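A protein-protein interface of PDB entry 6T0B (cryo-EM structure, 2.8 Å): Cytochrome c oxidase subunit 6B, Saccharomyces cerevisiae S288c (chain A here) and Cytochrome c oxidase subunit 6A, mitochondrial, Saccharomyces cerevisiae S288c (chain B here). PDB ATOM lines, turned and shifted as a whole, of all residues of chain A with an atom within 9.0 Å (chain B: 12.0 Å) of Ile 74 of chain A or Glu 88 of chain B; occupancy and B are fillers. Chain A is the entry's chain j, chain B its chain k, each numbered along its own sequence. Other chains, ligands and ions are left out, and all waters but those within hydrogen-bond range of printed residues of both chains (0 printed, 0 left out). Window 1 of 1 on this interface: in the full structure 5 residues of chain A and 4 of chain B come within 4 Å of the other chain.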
ATOM      1  N   ASP A  61      23.306  20.948  -5.144  1.00  0.00           N
ATOM      2  CA  ASP A  61      22.144  20.815  -4.267  1.00  0.00           C
ATOM      3  C   ASP A  61      22.246  19.573  -3.398  1.00  0.00           C
ATOM      4  O   ASP A  61      22.015  19.629  -2.186  1.00  0.00           O
ATOM      5  CB  ASP A  61      20.873  20.742  -5.119  1.00  0.00           C
ATOM      6  CG  ASP A  61      21.029  19.836  -6.332  1.00  0.00           C
ATOM      7  OD1 ASP A  61      20.151  19.856  -7.223  1.00  0.00           O
ATOM      8  OD2 ASP A  61      22.024  19.092  -6.397  1.00  0.00           O
ATOM      9  N   TRP A  62      22.671  18.465  -4.003  1.00  0.00           N
ATOM     10  CA  TRP A  62      22.801  17.205  -3.296  1.00  0.00           C
ATOM     11  C   TRP A  62      23.972  17.240  -2.330  1.00  0.00           C
ATOM     12  O   TRP A  62      23.880  16.691  -1.228  1.00  0.00           O
ATOM     13  CB  TRP A  62      22.988  16.062  -4.291  1.00  0.00           C
ATOM     14  CG  TRP A  62      21.810  15.726  -5.155  1.00  0.00           C
ATOM     15  CD1 TRP A  62      20.701  16.479  -5.373  1.00  0.00           C
ATOM     16  CD2 TRP A  62      21.652  14.548  -5.946  1.00  0.00           C
ATOM     17  NE1 TRP A  62      19.856  15.843  -6.239  1.00  0.00           N
ATOM     18  CE2 TRP A  62      20.417  14.653  -6.606  1.00  0.00           C
ATOM     19  CE3 TRP A  62      22.434  13.409  -6.155  1.00  0.00           C
ATOM     20  CZ2 TRP A  62      19.942  13.665  -7.456  1.00  0.00           C
ATOM     21  CZ3 TRP A  62      21.961  12.427  -7.000  1.00  0.00           C
ATOM     22  CH2 TRP A  62      20.729  12.562  -7.640  1.00  0.00           C
ATOM     23  N   LYS A  65      22.913  19.460   0.553  1.00  0.00           N
ATOM     24  CA  LYS A  65      21.879  18.745   1.291  1.00  0.00           C
ATOM     25  C   LYS A  65      22.482  17.654   2.158  1.00  0.00           C
ATOM     26  O   LYS A  65      22.122  17.517   3.330  1.00  0.00           O
ATOM     27  CB  LYS A  65      20.865  18.157   0.313  1.00  0.00           C
ATOM     28  CG  LYS A  65      19.643  17.544   0.958  1.00  0.00           C
ATOM     29  CD  LYS A  65      18.848  16.697  -0.021  1.00  0.00           C
ATOM     30  CE  LYS A  65      19.728  15.673  -0.715  1.00  0.00           C
ATOM     31  NZ  LYS A  65      18.982  14.455  -1.127  1.00  0.00           N
ATOM     32  N   TRP A  66      23.437  16.899   1.616  1.00  0.00           N
ATOM     33  CA  TRP A  66      24.037  15.816   2.377  1.00  0.00           C
ATOM     34  C   TRP A  66      24.959  16.331   3.473  1.00  0.00           C
ATOM     35  O   TRP A  66      25.059  15.706   4.534  1.00  0.00           O
ATOM     36  CB  TRP A  66      24.797  14.881   1.449  1.00  0.00           C
ATOM     37  CG  TRP A  66      23.932  14.111   0.525  1.00  0.00           C
ATOM     38  CD1 TRP A  66      22.586  13.953   0.604  1.00  0.00           C
ATOM     39  CD2 TRP A  66      24.356  13.389  -0.631  1.00  0.00           C
ATOM     40  NE1 TRP A  66      22.140  13.177  -0.435  1.00  0.00           N
ATOM     41  CE2 TRP A  66      23.212  12.818  -1.208  1.00  0.00           C
ATOM     42  CE3 TRP A  66      25.595  13.171  -1.235  1.00  0.00           C
ATOM     43  CZ2 TRP A  66      23.268  12.044  -2.360  1.00  0.00           C
ATOM     44  CZ3 TRP A  66      25.649  12.402  -2.372  1.00  0.00           C
ATOM     45  CH2 TRP A  66      24.493  11.848  -2.925  1.00  0.00           C
ATOM     46  N   ASP A  67      25.630  17.461   3.250  1.00  0.00           N
ATOM     47  CA  ASP A  67      26.469  18.020   4.304  1.00  0.00           C
ATOM     48  C   ASP A  67      25.616  18.608   5.417  1.00  0.00           C
ATOM     49  O   ASP A  67      25.950  18.475   6.608  1.00  0.00           O
ATOM     50  CB  ASP A  67      27.414  19.063   3.720  1.00  0.00           C
ATOM     51  CG  ASP A  67      28.516  18.443   2.894  1.00  0.00           C
ATOM     52  OD1 ASP A  67      28.914  17.302   3.196  1.00  0.00           O
ATOM     53  OD2 ASP A  67      28.994  19.097   1.950  1.00  0.00           O
ATOM     54  N   ASP A  68      24.479  19.204   5.049  1.00  0.00           N
ATOM     55  CA  ASP A  68      23.514  19.637   6.047  1.00  0.00           C
ATOM     56  C   ASP A  68      22.977  18.451   6.832  1.00  0.00           C
ATOM     57  O   ASP A  68      22.837  18.535   8.052  1.00  0.00           O
ATOM     58  CB  ASP A  68      22.365  20.387   5.374  1.00  0.00           C
ATOM     59  CG  ASP A  68      21.351  20.920   6.371  1.00  0.00           C
ATOM     60  OD1 ASP A  68      20.196  21.177   5.970  1.00  0.00           O
ATOM     61  OD2 ASP A  68      21.701  21.101   7.554  1.00  0.00           O
ATOM     62  N   GLN A  69      22.734  17.322   6.158  1.00  0.00           N
ATOM     63  CA  GLN A  69      22.181  16.153   6.833  1.00  0.00           C
ATOM     64  C   GLN A  69      23.195  15.481   7.748  1.00  0.00           C
ATOM     65  O   GLN A  69      22.823  14.951   8.806  1.00  0.00           O
ATOM     66  CB  GLN A  69      21.610  15.183   5.807  1.00  0.00           C
ATOM     67  CG  GLN A  69      20.281  15.669   5.311  1.00  0.00           C
ATOM     68  CD  GLN A  69      19.792  14.923   4.100  1.00  0.00           C
ATOM     69  OE1 GLN A  69      20.393  13.945   3.654  1.00  0.00           O
ATOM     70  NE2 GLN A  69      18.706  15.406   3.537  1.00  0.00           N
ATOM     71  N   ARG A  70      24.472  15.502   7.380  1.00  0.00           N
ATOM     72  CA  ARG A  70      25.478  14.986   8.295  1.00  0.00           C
ATOM     73  C   ARG A  70      25.707  15.919   9.480  1.00  0.00           C
ATOM     74  O   ARG A  70      26.133  15.447  10.543  1.00  0.00           O
ATOM     75  CB  ARG A  70      26.780  14.692   7.541  1.00  0.00           C
ATOM     76  CG  ARG A  70      27.735  15.832   7.419  1.00  0.00           C
ATOM     77  CD  ARG A  70      28.985  15.437   6.689  1.00  0.00           C
ATOM     78  NE  ARG A  70      29.821  16.607   6.445  1.00  0.00           N
ATOM     79  CZ  ARG A  70      30.707  17.083   7.312  1.00  0.00           C
ATOM     80  NH1 ARG A  70      30.882  16.488   8.483  1.00  0.00           N
ATOM     81  NH2 ARG A  70      31.419  18.158   7.009  1.00  0.00           N
ATOM     82  N   GLU A  71      25.400  17.216   9.351  1.00  0.00           N
ATOM     83  CA  GLU A  71      25.399  18.038  10.563  1.00  0.00           C
ATOM     84  C   GLU A  71      24.110  17.859  11.372  1.00  0.00           C
ATOM     85  O   GLU A  71      24.137  18.002  12.598  1.00  0.00           O
ATOM     86  CB  GLU A  71      25.654  19.511  10.219  1.00  0.00           C
ATOM     87  CG  GLU A  71      25.762  20.447  11.434  1.00  0.00           C
ATOM     88  CD  GLU A  71      26.866  21.488  11.337  1.00  0.00           C
ATOM     89  OE1 GLU A  71      27.544  21.732  12.363  1.00  0.00           O
ATOM     90  OE2 GLU A  71      27.047  22.071  10.250  1.00  0.00           O
ATOM     91  N   LYS A  72      22.998  17.505  10.717  1.00  0.00           N
ATOM     92  CA  LYS A  72      21.774  17.131  11.429  1.00  0.00           C
ATOM     93  C   LYS A  72      22.000  15.913  12.306  1.00  0.00           C
ATOM     94  O   LYS A  72      21.629  15.904  13.482  1.00  0.00           O
ATOM     95  CB  LYS A  72      20.657  16.744  10.475  1.00  0.00           C
ATOM     96  CG  LYS A  72      20.143  17.590   9.358  1.00  0.00           C
ATOM     97  CD  LYS A  72      19.160  18.677   9.561  1.00  0.00           C
ATOM     98  CE  LYS A  72      18.700  19.053   8.148  1.00  0.00           C
ATOM     99  NZ  LYS A  72      17.661  20.098   7.958  1.00  0.00           N
ATOM    100  N   GLY A  73      22.615  14.878  11.741  1.00  0.00           N
ATOM    101  CA  GLY A  73      22.422  13.529  12.226  1.00  0.00           C
ATOM    102  C   GLY A  73      21.364  12.775  11.460  1.00  0.00           C
ATOM    103  O   GLY A  73      20.891  11.735  11.926  1.00  0.00           O
ATOM    104  N   ILE A  74      20.981  13.281  10.295  1.00  0.00           N
ATOM    105  CA  ILE A  74      19.955  12.721   9.435  1.00  0.00           C
ATOM    106  C   ILE A  74      20.583  12.092   8.182  1.00  0.00           C
ATOM    107  O   ILE A  74      19.884  11.498   7.354  1.00  0.00           O
ATOM    108  CB  ILE A  74      18.894  13.820   9.164  1.00  0.00           C
ATOM    109  CG1 ILE A  74      18.231  14.157  10.502  1.00  0.00           C
ATOM    110  CG2 ILE A  74      17.752  13.521   8.201  1.00  0.00           C
ATOM    111  CD1 ILE A  74      17.666  12.957  11.244  1.00  0.00           C
ATOM    112  N   PHE A  75      21.913  12.089   8.091  1.00  0.00           N
ATOM    113  CA  PHE A  75      22.557  11.430   6.963  1.00  0.00           C
ATOM    114  C   PHE A  75      22.403   9.918   7.052  1.00  0.00           C
ATOM    115  O   PHE A  75      22.680   9.309   8.087  1.00  0.00           O
ATOM    116  CB  PHE A  75      24.035  11.785   6.871  1.00  0.00           C
ATOM    117  CG  PHE A  75      24.668  11.320   5.590  1.00  0.00           C
ATOM    118  CD1 PHE A  75      24.010  11.509   4.387  1.00  0.00           C
ATOM    119  CD2 PHE A  75      25.886  10.672   5.583  1.00  0.00           C
ATOM    120  CE1 PHE A  75      24.558  11.079   3.208  1.00  0.00           C
ATOM    121  CE2 PHE A  75      26.440  10.243   4.398  1.00  0.00           C
ATOM    122  CZ  PHE A  75      25.771  10.450   3.213  1.00  0.00           C
ATOM    123  N   ALA A  76      21.960   9.320   5.950  1.00  0.00           N
ATOM    124  CA  ALA A  76      21.641   7.904   5.876  1.00  0.00           C
ATOM    125  C   ALA A  76      22.838   7.027   5.508  1.00  0.00           C
ATOM    126  O   ALA A  76      22.640   5.883   5.094  1.00  0.00           O
ATOM    127  CB  ALA A  76      20.502   7.692   4.880  1.00  0.00           C
ATOM    128  N   GLY A  77      24.066   7.523   5.647  1.00  0.00           N
ATOM    129  CA  GLY A  77      25.248   6.702   5.523  1.00  0.00           C
ATOM    130  C   GLY A  77      25.910   6.465   6.873  1.00  0.00           C
ATOM    131  O   GLY A  77      25.473   6.948   7.913  1.00  0.00           O
ATOM    132  N   ILE A  79      29.229   7.293   8.458  1.00  0.00           N
ATOM    133  CA  ILE A  79      30.474   8.046   8.459  1.00  0.00           C
ATOM    134  C   ILE A  79      30.952   8.369   9.869  1.00  0.00           C
ATOM    135  O   ILE A  79      31.949   9.071  10.035  1.00  0.00           O
ATOM    136  CB  ILE A  79      30.352   9.326   7.610  1.00  0.00           C
ATOM    137  CG1 ILE A  79      29.284  10.267   8.181  1.00  0.00           C
ATOM    138  CG2 ILE A  79      30.023   8.966   6.187  1.00  0.00           C
ATOM    139  CD1 ILE A  79      29.286  11.656   7.546  1.00  0.00           C
ATOM    140  N   ASN A  80      30.274   7.851  10.888  1.00  0.00           N
ATOM    141  CA  ASN A  80      30.734   7.996  12.266  1.00  0.00           C
ATOM    142  C   ASN A  80      31.501   6.754  12.709  1.00  0.00           C
ATOM    143  O   ASN A  80      32.723   6.690  12.587  1.00  0.00           O
ATOM    144  CB  ASN A  80      29.555   8.248  13.210  1.00  0.00           C
ATOM    145  CG  ASN A  80      29.136   9.697  13.238  1.00  0.00           C
ATOM    146  OD1 ASN A  80      29.967  10.597  13.128  1.00  0.00           O
ATOM    147  ND2 ASN A  80      27.839   9.933  13.386  1.00  0.00           N
ATOM    148  N   ASP B  80       9.401  14.726  23.999  1.00  0.00           N
ATOM    149  CA  ASP B  80       9.716  14.824  22.580  1.00  0.00           C
ATOM    150  C   ASP B  80      11.052  15.495  22.273  1.00  0.00           C
ATOM    151  O   ASP B  80      11.489  15.449  21.120  1.00  0.00           O
ATOM    152  CB  ASP B  80       8.590  15.564  21.860  1.00  0.00           C
ATOM    153  CG  ASP B  80       8.190  16.828  22.571  1.00  0.00           C
ATOM    154  OD1 ASP B  80       8.631  17.020  23.721  1.00  0.00           O
ATOM    155  OD2 ASP B  80       7.436  17.631  21.981  1.00  0.00           O
ATOM    156  N   TRP B  83      13.167  12.471  22.031  1.00  0.00           N
ATOM    157  CA  TRP B  83      12.792  11.680  20.876  1.00  0.00           C
ATOM    158  C   TRP B  83      13.891  11.736  19.820  1.00  0.00           C
ATOM    159  O   TRP B  83      14.565  12.759  19.676  1.00  0.00           O
ATOM    160  CB  TRP B  83      11.489  12.209  20.289  1.00  0.00           C
ATOM    161  CG  TRP B  83      10.718  11.209  19.496  1.00  0.00           C
ATOM    162  CD1 TRP B  83      10.486  11.235  18.155  1.00  0.00           C
ATOM    163  CD2 TRP B  83      10.076  10.027  19.991  1.00  0.00           C
ATOM    164  NE1 TRP B  83       9.739  10.147  17.782  1.00  0.00           N
ATOM    165  CE2 TRP B  83       9.475   9.390  18.891  1.00  0.00           C
ATOM    166  CE3 TRP B  83       9.950   9.449  21.256  1.00  0.00           C
ATOM    167  CZ2 TRP B  83       8.764   8.204  19.017  1.00  0.00           C
ATOM    168  CZ3 TRP B  83       9.243   8.271  21.378  1.00  0.00           C
ATOM    169  CH2 TRP B  83       8.660   7.660  20.264  1.00  0.00           C
ATOM    170  N   PRO B  84      14.110  10.646  19.083  1.00  0.00           N
ATOM    171  CA  PRO B  84      15.068  10.696  17.975  1.00  0.00           C
ATOM    172  C   PRO B  84      14.534  11.528  16.823  1.00  0.00           C
ATOM    173  O   PRO B  84      13.354  11.458  16.477  1.00  0.00           O
ATOM    174  CB  PRO B  84      15.224   9.226  17.576  1.00  0.00           C
ATOM    175  CG  PRO B  84      13.987   8.588  18.036  1.00  0.00           C
ATOM    176  CD  PRO B  84      13.623   9.277  19.306  1.00  0.00           C
ATOM    177  N   ARG B  85      15.421  12.334  16.244  1.00  0.00           N
ATOM    178  CA  ARG B  85      15.047  13.235  15.166  1.00  0.00           C
ATOM    179  C   ARG B  85      14.695  12.449  13.911  1.00  0.00           C
ATOM    180  O   ARG B  85      15.384  11.492  13.548  1.00  0.00           O
ATOM    181  CB  ARG B  85      16.194  14.205  14.887  1.00  0.00           C
ATOM    182  CG  ARG B  85      15.930  15.213  13.795  1.00  0.00           C
ATOM    183  CD  ARG B  85      17.109  16.143  13.621  1.00  0.00           C
ATOM    184  NE  ARG B  85      17.285  17.021  14.770  1.00  0.00           N
ATOM    185  CZ  ARG B  85      18.340  17.811  14.946  1.00  0.00           C
ATOM    186  NH1 ARG B  85      19.317  17.824  14.045  1.00  0.00           N
ATOM    187  NH2 ARG B  85      18.424  18.583  16.020  1.00  0.00           N
ATOM    188  N   ASP B  86      13.602  12.845  13.261  1.00  0.00           N
ATOM    189  CA  ASP B  86      13.116  12.116  12.097  1.00  0.00           C
ATOM    190  C   ASP B  86      14.048  12.291  10.908  1.00  0.00           C
ATOM    191  O   ASP B  86      14.517  13.394  10.626  1.00  0.00           O
ATOM    192  CB  ASP B  86      11.720  12.601  11.708  1.00  0.00           C
ATOM    193  CG  ASP B  86      10.664  12.208  12.707  1.00  0.00           C
ATOM    194  OD1 ASP B  86      10.830  11.167  13.376  1.00  0.00           O
ATOM    195  OD2 ASP B  86       9.659  12.939  12.817  1.00  0.00           O
ATOM    196  N   TYR B  87      14.268  11.200  10.179  1.00  0.00           N
ATOM    197  CA  TYR B  87      15.020  11.251   8.936  1.00  0.00           C
ATOM    198  C   TYR B  87      14.231  12.022   7.875  1.00  0.00           C
ATOM    199  O   TYR B  87      13.065  12.385   8.065  1.00  0.00           O
ATOM    200  CB  TYR B  87      15.362   9.841   8.460  1.00  0.00           C
ATOM    201  CG  TYR B  87      16.582   9.228   9.122  1.00  0.00           C
ATOM    202  CD1 TYR B  87      17.855   9.510   8.663  1.00  0.00           C
ATOM    203  CD2 TYR B  87      16.456   8.358  10.196  1.00  0.00           C
ATOM    204  CE1 TYR B  87      18.970   8.962   9.260  1.00  0.00           C
ATOM    205  CE2 TYR B  87      17.569   7.801  10.798  1.00  0.00           C
ATOM    206  CZ  TYR B  87      18.821   8.109  10.324  1.00  0.00           C
ATOM    207  OH  TYR B  87      19.934   7.559  10.916  1.00  0.00           O
ATOM    208  N   GLU B  88      14.890  12.276   6.740  1.00  0.00           N
ATOM    209  CA  GLU B  88      14.327  13.134   5.697  1.00  0.00           C
ATOM    210  C   GLU B  88      13.058  12.551   5.094  1.00  0.00           C
ATOM    211  O   GLU B  88      12.113  13.289   4.791  1.00  0.00           O
ATOM    212  CB  GLU B  88      15.364  13.353   4.596  1.00  0.00           C
ATOM    213  CG  GLU B  88      14.903  14.262   3.476  1.00  0.00           C
ATOM    214  CD  GLU B  88      15.939  14.433   2.395  1.00  0.00           C
ATOM    215  OE1 GLU B  88      17.006  13.791   2.489  1.00  0.00           O
ATOM    216  OE2 GLU B  88      15.702  15.226   1.463  1.00  0.00           O
ATOM    217  N   PHE B  89      12.998  11.238   4.965  1.00  0.00           N
ATOM    218  CA  PHE B  89      11.858  10.585   4.353  1.00  0.00           C
ATOM    219  C   PHE B  89      10.714  10.343   5.324  1.00  0.00           C
ATOM    220  O   PHE B  89       9.628   9.959   4.883  1.00  0.00           O
ATOM    221  CB  PHE B  89      12.295   9.258   3.721  1.00  0.00           C
ATOM    222  CG  PHE B  89      13.089   8.370   4.634  1.00  0.00           C
ATOM    223  CD1 PHE B  89      12.454   7.447   5.441  1.00  0.00           C
ATOM    224  CD2 PHE B  89      14.472   8.433   4.664  1.00  0.00           C
ATOM    225  CE1 PHE B  89      13.171   6.634   6.273  1.00  0.00           C
ATOM    226  CE2 PHE B  89      15.192   7.618   5.498  1.00  0.00           C
ATOM    227  CZ  PHE B  89      14.539   6.719   6.297  1.00  0.00           C
ATOM    228  N   MET B  90      10.914  10.552   6.618  1.00  0.00           N
ATOM    229  CA  MET B  90       9.905  10.195   7.602  1.00  0.00           C
ATOM    230  C   MET B  90       8.900  11.323   7.769  1.00  0.00           C
ATOM    231  O   MET B  90       9.285  12.491   7.865  1.00  0.00           O
ATOM    232  CB  MET B  90      10.562   9.858   8.934  1.00  0.00           C
ATOM    233  CG  MET B  90      11.780   8.984   8.778  1.00  0.00           C
ATOM    234  SD  MET B  90      12.458   8.404  10.337  1.00  0.00           S
ATOM    235  CE  MET B  90      11.242   7.175  10.796  1.00  0.00           C
ATOM    236  N   ASN B  91       7.615  10.954   7.798  1.00  0.00           N
ATOM    237  CA  ASN B  91       6.467  11.851   7.964  1.00  0.00           C
ATOM    238  C   ASN B  91       6.431  12.923   6.871  1.00  0.00           C
ATOM    239  O   ASN B  91       6.627  14.115   7.105  1.00  0.00           O
ATOM    240  CB  ASN B  91       6.433  12.467   9.367  1.00  0.00           C
ATOM    241  CG  ASN B  91       6.040  11.462  10.423  1.00  0.00           C
ATOM    242  OD1 ASN B  91       5.141  10.648  10.216  1.00  0.00           O
ATOM    243  ND2 ASN B  91       6.714  11.508  11.561  1.00  0.00           N
ATOM    244  N   ILE B  92       6.195  12.430   5.654  1.00  0.00           N
ATOM    245  CA  ILE B  92       6.027  13.292   4.492  1.00  0.00           C
ATOM    246  C   ILE B  92       4.783  14.144   4.665  1.00  0.00           C
ATOM    247  O   ILE B  92       3.698  13.633   4.969  1.00  0.00           O
ATOM    248  CB  ILE B  92       5.941  12.433   3.222  1.00  0.00           C
ATOM    249  CG1 ILE B  92       7.252  11.680   2.985  1.00  0.00           C
ATOM    250  CG2 ILE B  92       5.572  13.274   2.018  1.00  0.00           C
ATOM    251  CD1 ILE B  92       8.492  12.536   3.055  1.00  0.00           C
ATOM    252  N   ARG B  93       4.937  15.463   4.498  1.00  0.00           N
ATOM    253  CA  ARG B  93       3.822  16.411   4.594  1.00  0.00           C
ATOM    254  C   ARG B  93       3.812  17.262   3.328  1.00  0.00           C
ATOM    255  O   ARG B  93       4.377  18.355   3.292  1.00  0.00           O
ATOM    256  CB  ARG B  93       3.934  17.263   5.843  1.00  0.00           C
ATOM    257  CG  ARG B  93       3.835  16.479   7.124  1.00  0.00           C
ATOM    258  CD  ARG B  93       2.472  15.848   7.278  1.00  0.00           C
ATOM    259  NE  ARG B  93       2.337  15.227   8.587  1.00  0.00           N
ATOM    260  CZ  ARG B  93       2.251  13.920   8.786  1.00  0.00           C
ATOM    261  NH1 ARG B  93       2.264  13.097   7.755  1.00  0.00           N
ATOM    262  NH2 ARG B  93       2.137  13.440  10.011  1.00  0.00           N
ATOM    263  N   SER B  94       3.161  16.753   2.286  1.00  0.00           N
ATOM    264  CA  SER B  94       3.020  17.517   1.055  1.00  0.00           C
ATOM    265  C   SER B  94       1.905  18.545   1.185  1.00  0.00           C
ATOM    266  O   SER B  94       2.131  19.751   1.046  1.00  0.00           O
ATOM    267  CB  SER B  94       2.760  16.568  -0.113  1.00  0.00           C
ATOM    268  OG  SER B  94       1.598  15.794   0.118  1.00  0.00           O
ATOM    269  N   ARG B 114       5.150  10.155  16.525  1.00  0.00           N
ATOM    270  CA  ARG B 114       5.325  11.532  16.964  1.00  0.00           C
ATOM    271  C   ARG B 114       5.961  12.336  15.844  1.00  0.00           C
ATOM    272  O   ARG B 114       6.969  11.913  15.272  1.00  0.00           O
ATOM    273  CB  ARG B 114       6.190  11.602  18.226  1.00  0.00           C
ATOM    274  CG  ARG B 114       5.399  11.566  19.527  1.00  0.00           C
ATOM    275  CD  ARG B 114       6.270  11.169  20.696  1.00  0.00           C
ATOM    276  NE  ARG B 114       5.491  10.996  21.912  1.00  0.00           N
ATOM    277  CZ  ARG B 114       5.994  10.576  23.063  1.00  0.00           C
ATOM    278  NH1 ARG B 114       5.209  10.449  24.122  1.00  0.00           N
ATOM    279  NH2 ARG B 114       7.279  10.286  23.160  1.00  0.00           N
ATOM    280  N   HIS B 115       5.377  13.491  15.539  1.00  0.00           N
ATOM    281  CA  HIS B 115       5.880  14.393  14.507  1.00  0.00           C
ATOM    282  C   HIS B 115       6.242  15.720  15.158  1.00  0.00           C
ATOM    283  O   HIS B 115       5.355  16.498  15.524  1.00  0.00           O
ATOM    284  CB  HIS B 115       4.843  14.595  13.409  1.00  0.00           C
ATOM    285  CG  HIS B 115       5.310  15.471  12.292  1.00  0.00           C
ATOM    286  ND1 HIS B 115       4.471  16.340  11.630  1.00  0.00           N
ATOM    287  CD2 HIS B 115       6.526  15.607  11.714  1.00  0.00           C
ATOM    288  CE1 HIS B 115       5.151  16.976  10.696  1.00  0.00           C
ATOM    289  NE2 HIS B 115       6.401  16.551  10.725  1.00  0.00           N
ATOM    290  N   ILE B 116       7.537  15.983  15.287  1.00  0.00           N
ATOM    291  CA  ILE B 116       8.023  17.171  15.977  1.00  0.00           C
ATOM    292  C   ILE B 116       8.726  18.117  15.010  1.00  0.00           C
ATOM    293  O   ILE B 116       8.425  19.310  14.954  1.00  0.00           O
ATOM    294  CB  ILE B 116       8.961  16.786  17.130  1.00  0.00           C
ATOM    295  CG1 ILE B 116       8.206  15.998  18.195  1.00  0.00           C
ATOM    296  CG2 ILE B 116       9.601  18.018  17.742  1.00  0.00           C
ATOM    297  CD1 ILE B 116       8.490  14.527  18.187  1.00  0.00           C
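Of the 17 printed residues of chain A, 5 touch a printed residue of chain B. Of the 16 printed residues of chain B, 4 touch a printed residue of chain A. Printed residues of chain B that touch a printed residue of chain A: Arg 85, Asp 86, Tyr 87 and Glu 88.
The backbone carbonyl oxygen (O) of Lys 72 of chain A is in hydrogen-bond range of the guanidinium group (NH1) of Arg 85 of chain B (3.1 Å). NE2 of Gln 69 of chain A is in hydrogen-bond range of OE1 of Glu 88 of chain B, at 2.6 Å.
Among the printed residues, pairs that only touch across the chains: Ile 74 of chain A with Tyr 87 of chain B (3.1 Å), Ile 74 of chain A with Asp 86 of chain B (3.2 Å), Ile 74 of chain A with Glu 88 of chain B (3.4 Å), Ile 74 of chain A with Arg 85 of chain B (3.6 Å), Lys 65 of chain A with Glu 88 of chain B (3.8 Å) and Phe 75 of chain A with Tyr 87 of chain B (3.9 Å).
Printed residues of chain B within 4 Å of Lys 65 of chain A: Glu 88 (3.8 Å). Gln 69 of chain A touches just one residue of chain B: Glu 88 (2.6 Å). Glu 71 of chain A touches none of the printed residues of chain B. Of chain B, only Arg 85 (3.1 Å) comes within 4 Å of Lys 72 of chain A. Gly 73 of chain A touches none of the printed residues of chain B. Phe 75 of chain A touches just one residue of chain B: Tyr 87. No residue of chain B comes within 4 Å of Ala 76 of chain A. Of the printed residues of chain A, Arg 85 of chain B touches Lys 72 and Ile 74. Of the printed residues of chain A, Tyr 87 of chain B touches Ile 74 and Phe 75. Asn 91 of chain B touches none of the printed residues of chain A. The nearest residue of chain B that does not touch Ile 74 of chain A is Phe 89 of chain B (6.2 Å). The nearest printed residue of chain A that does not touch Asp 86 of chain B is Gly 73 of chain A (6.7 Å).
N of Phe 75 of chain A lies within hydrogen-bond range of O of Gln 69 of chain A. O of Gln 69 of chain A sits at hydrogen-bond distance from N of Ile 74 of chain A (2.9 Å). The side-chain sulfur (SD) of Met 90 of chain B lies within hydrogen-bond range of the backbone NH (N) of Tyr 87 of chain B (3.3 Å). The side-chain amino group of Lys 72 of chain A lies within salt-bridge range of the side-chain carboxylate of Asp 68 of chain A, 3.4 Å away.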
